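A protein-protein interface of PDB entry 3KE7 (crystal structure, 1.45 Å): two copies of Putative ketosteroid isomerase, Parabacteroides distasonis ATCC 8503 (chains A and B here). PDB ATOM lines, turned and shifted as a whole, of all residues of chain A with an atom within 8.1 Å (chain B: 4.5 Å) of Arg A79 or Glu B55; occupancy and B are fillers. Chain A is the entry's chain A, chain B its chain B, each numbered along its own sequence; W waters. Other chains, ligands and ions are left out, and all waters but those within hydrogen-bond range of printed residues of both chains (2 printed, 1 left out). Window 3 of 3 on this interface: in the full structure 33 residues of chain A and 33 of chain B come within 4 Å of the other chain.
Ile A20 touches none of the printed residues of chain B.
Met A77 touches none of the printed residues of chain B.
Printed residues of chain B within 4 Å of Arg A79: Thr B52, Lys B53 and Glu B55.
Printed residues of chain B within 4 Å of Val A81: Lys B53 and Glu B55.
Of the printed residues of chain B, Asn A94 touches Thr B52 (3.1 Å) and Lys B53 (3.1 Å).
Of the printed residues of chain A, Ile B44 touches Thr A92 (3.4 Å).
Of the printed residues of chain A, Glu B55 touches Arg A79 (2.6 Å) and Val A81 (3.9 Å).
Of the 8 printed residues of chain B, 4 touch a printed residue of chain A.
Hydrophobic or aromatic side chains of chain B that line the printed part of chain A: Ile B44.
Of the 13 printed residues of chain A, 4 touch a printed residue of chain B.
Hydrophobic or aromatic side chains of chain A within 4 Å of the printed part of chain B: Val A81.
Among the printed residues, 9 pairs touch across the chains.
Among the printed residues, Asp or Glu carboxylates within 4 Å of a Lys or Arg side-chain nitrogen of the other chain: Arg A79 with Glu B55 (2.6 Å).
No position is printed for both chains.
Of the 9 pairs that touch across the chains among the printed residues, none has its exchanged pair printed and touching as well.
NH2 of Arg A79 sits at hydrogen-bond distance from OG1 of Thr B52, at 3.1 Å.
The side-chain amino group (NZ) of Lys B53 is in hydrogen-bond range of the backbone carbonyl oxygen (O) of Arg A79 (2.7 Å).
OE2 of Glu B55 lies within salt-bridge range of NE of Arg A79, at 2.6 Å.
OD1 of Asn A94 is in hydrogen-bond range of OG1 of Thr B52 (3.1 Å).
N of Lys B53 sits at hydrogen-bond distance from OD1 of Asn A94 (3.1 Å).
Val A81 touches Lys B53.
Val A81 touches Glu B55 (CG2 to OE1, 3.9 Å).
CG2 of Ile B44 touches OG1 of Thr A92, 3.4 Å away.
Lys B53 touches Thr A92 (CE to OG1, 3.5 Å).
Water W1 lies within hydrogen-bond range of the side-chain amide oxygen of Asn A94 (2.7 Å), the side-chain amino group of Lys B53 (2.7 Å), the backbone carbonyl oxygen of Ile A78 (2.8 Å) and the guanidinium group of Arg A79 (3.5 Å).
Water W2 bridges the side-chain hydroxyl (OG1) of Thr B52 (2.8 Å) and the side-chain amide oxygen (OD1) of Asn A94 (3.4 Å).
The backbone NH of Ile A78 is in hydrogen-bond range of the backbone carbonyl oxygen of Asn A94 (2.8 Å).
The backbone NH (N) of Val A81 lies within hydrogen-bond range of the backbone carbonyl oxygen (O) of Thr A92 (2.8 Å).
The side-chain amino group of Lys B53 lies within salt-bridge range of the side-chain carboxylate of Glu B55.
The side-chain amide oxygen (OE1) of Gln B59 is in hydrogen-bond range of the backbone NH (N) of Glu B55, 2.8 Å away.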
ATOM      1  N   ILE A  20     -15.841  17.339  22.409  1.00  0.00           N
ATOM      2  CA  ILE A  20     -15.679  16.817  21.047  1.00  0.00           C
ATOM      3  C   ILE A  20     -15.956  17.912  20.011  1.00  0.00           C
ATOM      4  O   ILE A  20     -15.179  18.081  19.059  1.00  0.00           O
ATOM      5  CB  ILE A  20     -16.561  15.592  20.847  1.00  0.00           C
ATOM      6  CG1 ILE A  20     -16.020  14.435  21.691  1.00  0.00           C
ATOM      7  CG2 ILE A  20     -16.689  15.230  19.323  1.00  0.00           C
ATOM      8  CD1 ILE A  20     -17.034  13.288  21.829  1.00  0.00           C
ATOM      9  N   ASP A  76     -11.727  12.963   9.552  1.00  0.00           N
ATOM     10  CA  ASP A  76     -12.643  12.059  10.240  1.00  0.00           C
ATOM     11  C   ASP A  76     -12.100  11.786  11.615  1.00  0.00           C
ATOM     12  O   ASP A  76     -10.985  11.244  11.773  1.00  0.00           O
ATOM     13  CB  ASP A  76     -12.776  10.759   9.475  1.00  0.00           C
ATOM     14  CG  ASP A  76     -13.319  10.973   8.079  1.00  0.00           C
ATOM     15  OD1 ASP A  76     -14.462  11.481   7.971  1.00  0.00           O
ATOM     16  OD2 ASP A  76     -12.639  10.668   7.124  1.00  0.00           O
ATOM     17  N   MET A  77     -12.860  12.174  12.639  1.00  0.00           N
ATOM     18  CA  MET A  77     -12.490  11.903  14.010  1.00  0.00           C
ATOM     19  C   MET A  77     -13.136  10.545  14.338  1.00  0.00           C
ATOM     20  O   MET A  77     -14.350  10.379  14.253  1.00  0.00           O
ATOM     21  CB  MET A  77     -12.972  13.025  14.914  1.00  0.00           C
ATOM     22  CG  MET A  77     -12.684  12.796  16.341  1.00  0.00           C
ATOM     23  SD  MET A  77     -13.159  14.209  17.533  1.00  0.00           S
ATOM     24  CE  MET A  77     -11.869  15.535  16.882  1.00  0.00           C
ATOM     25  N   ILE A  78     -12.305   9.578  14.700  1.00  0.00           N
ATOM     26  CA  ILE A  78     -12.734   8.228  14.923  1.00  0.00           C
ATOM     27  C   ILE A  78     -12.734   7.879  16.411  1.00  0.00           C
ATOM     28  O   ILE A  78     -11.715   8.020  17.140  1.00  0.00           O
ATOM     29  CB  ILE A  78     -11.792   7.262  14.205  1.00  0.00           C
ATOM     30  CG1 ILE A  78     -11.765   7.572  12.703  1.00  0.00           C
ATOM     31  CG2 ILE A  78     -12.157   5.777  14.465  1.00  0.00           C
ATOM     32  CD1 ILE A  78     -10.654   6.870  11.917  1.00  0.00           C
ATOM     33  N   ARG A  79     -13.902   7.457  16.843  1.00  0.00           N
ATOM     34  CA  ARG A  79     -14.180   6.986  18.157  1.00  0.00           C
ATOM     35  C   ARG A  79     -13.619   7.896  19.308  1.00  0.00           C
ATOM     36  O   ARG A  79     -12.926   7.453  20.197  1.00  0.00           O
ATOM     37  CB  ARG A  79     -13.665   5.537  18.217  1.00  0.00           C
ATOM     38  CG  ARG A  79     -14.538   4.645  18.932  1.00  0.00           C
ATOM     39  CD  ARG A  79     -14.163   3.215  18.763  1.00  0.00           C
ATOM     40  NE  ARG A  79     -12.830   2.945  19.255  1.00  0.00           N
ATOM     41  CZ  ARG A  79     -11.727   2.851  18.500  1.00  0.00           C
ATOM     42  NH1 ARG A  79     -11.779   2.949  17.162  1.00  0.00           N
ATOM     43  NH2 ARG A  79     -10.551   2.635  19.097  1.00  0.00           N
ATOM     44  N   PRO A  80     -13.961   9.195  19.280  1.00  0.00           N
ATOM     45  CA  PRO A  80     -13.535  10.060  20.358  1.00  0.00           C
ATOM     46  C   PRO A  80     -14.062   9.578  21.715  1.00  0.00           C
ATOM     47  O   PRO A  80     -15.249   9.215  21.802  1.00  0.00           O
ATOM     48  CB  PRO A  80     -14.133  11.422  19.992  1.00  0.00           C
ATOM     49  CG  PRO A  80     -15.309  11.109  19.123  1.00  0.00           C
ATOM     50  CD  PRO A  80     -14.936   9.865  18.387  1.00  0.00           C
ATOM     51  N   VAL A  81     -13.197   9.576  22.716  1.00  0.00           N
ATOM     52  CA  VAL A  81     -13.546   9.236  24.083  1.00  0.00           C
ATOM     53  C   VAL A  81     -13.251  10.411  24.979  1.00  0.00           C
ATOM     54  O   VAL A  81     -12.180  11.022  24.859  1.00  0.00           O
ATOM     55  CB  VAL A  81     -12.768   7.991  24.593  1.00  0.00           C
ATOM     56  CG1 VAL A  81     -12.978   7.765  26.106  1.00  0.00           C
ATOM     57  CG2 VAL A  81     -13.172   6.741  23.802  1.00  0.00           C
ATOM     58  N   VAL A  82     -14.195  10.774  25.847  1.00  0.00           N
ATOM     59  CA  VAL A  82     -13.954  11.800  26.831  1.00  0.00           C
ATOM     60  C   VAL A  82     -14.190  11.239  28.187  1.00  0.00           C
ATOM     61  O   VAL A  82     -15.265  10.740  28.506  1.00  0.00           O
ATOM     62  CB  VAL A  82     -14.852  13.048  26.618  1.00  0.00           C
ATOM     63  CG1 VAL A  82     -14.437  14.158  27.578  1.00  0.00           C
ATOM     64  CG2 VAL A  82     -14.726  13.588  25.204  1.00  0.00           C
ATOM     65  N   LEU A  91      -9.702  14.010  26.393  1.00  0.00           N
ATOM     66  CA  LEU A  91     -10.218  13.614  25.094  1.00  0.00           C
ATOM     67  C   LEU A  91      -9.144  12.840  24.340  1.00  0.00           C
ATOM     68  O   LEU A  91      -8.012  13.315  24.185  1.00  0.00           O
ATOM     69  CB  LEU A  91     -10.575  14.864  24.289  1.00  0.00           C
ATOM     70  CG  LEU A  91     -10.825  14.697  22.800  1.00  0.00           C
ATOM     71  CD1 LEU A  91     -12.082  13.868  22.517  1.00  0.00           C
ATOM     72  CD2 LEU A  91     -10.975  16.106  22.110  1.00  0.00           C
ATOM     73  N   THR A  92      -9.502  11.649  23.885  1.00  0.00           N
ATOM     74  CA  THR A  92      -8.642  10.829  23.066  1.00  0.00           C
ATOM     75  C   THR A  92      -9.358  10.429  21.783  1.00  0.00           C
ATOM     76  O   THR A  92     -10.575  10.158  21.787  1.00  0.00           O
ATOM     77  CB  THR A  92      -8.168   9.589  23.827  1.00  0.00           C
ATOM     78  OG1 THR A  92      -9.296   8.863  24.355  1.00  0.00           O
ATOM     79  CG2 THR A  92      -7.166   9.935  24.961  1.00  0.00           C
ATOM     80  N   PHE A  93      -8.622  10.418  20.680  1.00  0.00           N
ATOM     81  CA  PHE A  93      -9.207  10.011  19.402  1.00  0.00           C
ATOM     82  C   PHE A  93      -8.152   9.641  18.417  1.00  0.00           C
ATOM     83  O   PHE A  93      -6.971   9.932  18.610  1.00  0.00           O
ATOM     84  CB  PHE A  93     -10.105  11.139  18.841  1.00  0.00           C
ATOM     85  CG  PHE A  93      -9.425  12.466  18.644  1.00  0.00           C
ATOM     86  CD1 PHE A  93      -9.367  13.364  19.689  1.00  0.00           C
ATOM     87  CD2 PHE A  93      -8.900  12.838  17.415  1.00  0.00           C
ATOM     88  CE1 PHE A  93      -8.799  14.588  19.529  1.00  0.00           C
ATOM     89  CE2 PHE A  93      -8.310  14.077  17.236  1.00  0.00           C
ATOM     90  CZ  PHE A  93      -8.243  14.943  18.316  1.00  0.00           C
ATOM     91  N   ASN A  94      -8.588   8.932  17.384  1.00  0.00           N
ATOM     92  CA  ASN A  94      -7.819   8.829  16.168  1.00  0.00           C
ATOM     93  C   ASN A  94      -8.392   9.803  15.146  1.00  0.00           C
ATOM     94  O   ASN A  94      -9.573  10.151  15.180  1.00  0.00           O
ATOM     95  CB  ASN A  94      -7.824   7.402  15.650  1.00  0.00           C
ATOM     96  CG  ASN A  94      -6.982   6.458  16.533  1.00  0.00           C
ATOM     97  OD1 ASN A  94      -7.517   5.705  17.384  1.00  0.00           O
ATOM     98  ND2 ASN A  94      -5.669   6.558  16.403  1.00  0.00           N
ATOM     99  N   LEU A  95      -7.545  10.220  14.204  1.00  0.00           N
ATOM    100  CA  LEU A  95      -7.921  11.212  13.215  1.00  0.00           C
ATOM    101  C   LEU A  95      -7.380  10.874  11.856  1.00  0.00           C
ATOM    102  O   LEU A  95      -6.200  10.671  11.699  1.00  0.00           O
ATOM    103  CB  LEU A  95      -7.437  12.596  13.613  1.00  0.00           C
ATOM    104  CG  LEU A  95      -7.978  13.756  12.777  1.00  0.00           C
ATOM    105  CD1 LEU A  95      -9.374  14.074  13.161  1.00  0.00           C
ATOM    106  CD2 LEU A  95      -7.076  14.978  12.984  1.00  0.00           C
ATOM    107  N   VAL B  43      -9.055   2.745  31.184  1.00  0.00           N
ATOM    108  CA  VAL B  43      -7.841   3.258  30.591  1.00  0.00           C
ATOM    109  C   VAL B  43      -7.921   3.289  29.050  1.00  0.00           C
ATOM    110  O   VAL B  43      -8.472   2.398  28.423  1.00  0.00           O
ATOM    111  CB  VAL B  43      -6.636   2.422  31.076  1.00  0.00           C
ATOM    112  CG1 VAL B  43      -6.742   0.924  30.554  1.00  0.00           C
ATOM    113  CG2 VAL B  43      -5.318   3.057  30.674  1.00  0.00           C
ATOM    114  N   ILE B  44      -7.342   4.329  28.483  1.00  0.00           N
ATOM    115  CA  ILE B  44      -7.159   4.492  27.065  1.00  0.00           C
ATOM    116  C   ILE B  44      -5.651   4.518  26.847  1.00  0.00           C
ATOM    117  O   ILE B  44      -4.926   5.205  27.538  1.00  0.00           O
ATOM    118  CB  ILE B  44      -7.788   5.820  26.560  1.00  0.00           C
ATOM    119  CG1 ILE B  44      -9.275   5.910  26.873  1.00  0.00           C
ATOM    120  CG2 ILE B  44      -7.504   6.036  25.068  1.00  0.00           C
ATOM    121  CD1 ILE B  44     -10.088   4.899  26.253  1.00  0.00           C
ATOM    122  N   THR B  52      -5.262   1.633  16.031  1.00  0.00           N
ATOM    123  CA  THR B  52      -6.296   2.430  16.713  1.00  0.00           C
ATOM    124  C   THR B  52      -6.068   2.292  18.217  1.00  0.00           C
ATOM    125  O   THR B  52      -5.445   1.301  18.670  1.00  0.00           O
ATOM    126  CB  THR B  52      -7.707   1.942  16.271  1.00  0.00           C
ATOM    127  OG1 THR B  52      -8.647   2.901  16.693  1.00  0.00           O
ATOM    128  CG2 THR B  52      -8.042   0.552  16.861  1.00  0.00           C
ATOM    129  N   LYS B  53      -6.526   3.260  18.977  1.00  0.00           N
ATOM    130  CA  LYS B  53      -6.251   3.239  20.399  1.00  0.00           C
ATOM    131  C   LYS B  53      -6.898   2.040  21.125  1.00  0.00           C
ATOM    132  O   LYS B  53      -7.949   1.512  20.714  1.00  0.00           O
ATOM    133  CB  LYS B  53      -6.662   4.560  21.097  1.00  0.00           C
ATOM    134  CG  LYS B  53      -8.185   4.771  21.221  1.00  0.00           C
ATOM    135  CD  LYS B  53      -8.466   6.184  21.520  1.00  0.00           C
ATOM    136  CE  LYS B  53      -9.913   6.478  21.879  1.00  0.00           C
ATOM    137  NZ  LYS B  53     -10.860   5.922  20.865  1.00  0.00           N
ATOM    138  N   ILE B  54      -6.223   1.578  22.167  1.00  0.00           N
ATOM    139  CA  ILE B  54      -6.715   0.599  23.099  1.00  0.00           C
ATOM    140  C   ILE B  54      -7.661   1.258  24.055  1.00  0.00           C
ATOM    141  O   ILE B  54      -7.414   2.346  24.525  1.00  0.00           O
ATOM    142  CB  ILE B  54      -5.534  -0.099  23.834  1.00  0.00           C
ATOM    143  CG1 ILE B  54      -4.951  -1.155  22.926  1.00  0.00           C
ATOM    144  CG2 ILE B  54      -6.006  -0.703  25.174  1.00  0.00           C
ATOM    145  CD1 ILE B  54      -3.649  -1.823  23.457  1.00  0.00           C
ATOM    146  N   GLU B  55      -8.765   0.570  24.313  1.00  0.00           N
ATOM    147  CA  GLU B  55      -9.817   1.055  25.240  1.00  0.00           C
ATOM    148  C   GLU B  55     -10.190  -0.012  26.215  1.00  0.00           C
ATOM    149  O   GLU B  55     -10.753  -1.087  25.849  1.00  0.00           O
ATOM    150  CB  GLU B  55     -11.044   1.467  24.485  1.00  0.00           C
ATOM    151  CG  GLU B  55     -10.758   2.554  23.538  1.00  0.00           C
ATOM    152  CD  GLU B  55     -11.925   2.952  22.695  1.00  0.00           C
ATOM    153  OE1 GLU B  55     -13.101   2.918  23.196  1.00  0.00           O
ATOM    154  OE2 GLU B  55     -11.641   3.353  21.519  1.00  0.00           O
ATOM    155  N   GLY B  56      -9.997   0.305  27.469  1.00  0.00           N
ATOM    156  CA  GLY B  56     -10.346  -0.570  28.552  1.00  0.00           C
ATOM    157  C   GLY B  56      -9.207  -1.422  29.046  1.00  0.00           C
ATOM    158  O   GLY B  56      -8.340  -1.827  28.292  1.00  0.00           O
ATOM    159  N   GLN B  59      -8.536  -4.914  27.298  1.00  0.00           N
ATOM    160  CA  GLN B  59      -7.768  -4.789  26.047  1.00  0.00           C
ATOM    161  C   GLN B  59      -6.314  -4.497  26.343  1.00  0.00           C
ATOM    162  O   GLN B  59      -5.414  -5.049  25.693  1.00  0.00           O
ATOM    163  CB  GLN B  59      -8.286  -3.688  25.143  1.00  0.00           C
ATOM    164  CG  GLN B  59      -9.422  -4.078  24.242  1.00  0.00           C
ATOM    165  CD  GLN B  59      -9.821  -2.960  23.298  1.00  0.00           C
ATOM    166  OE1 GLN B  59      -9.091  -1.972  23.119  1.00  0.00           O
ATOM    167  NE2 GLN B  59     -10.994  -3.099  22.688  1.00  0.00           N
HETATM  168  O   HOH W   1     -10.063   5.983  18.234  1.00  0.00           O
HETATM  169  O   HOH W   2      -8.639   4.530  14.446  1.00  0.00           O
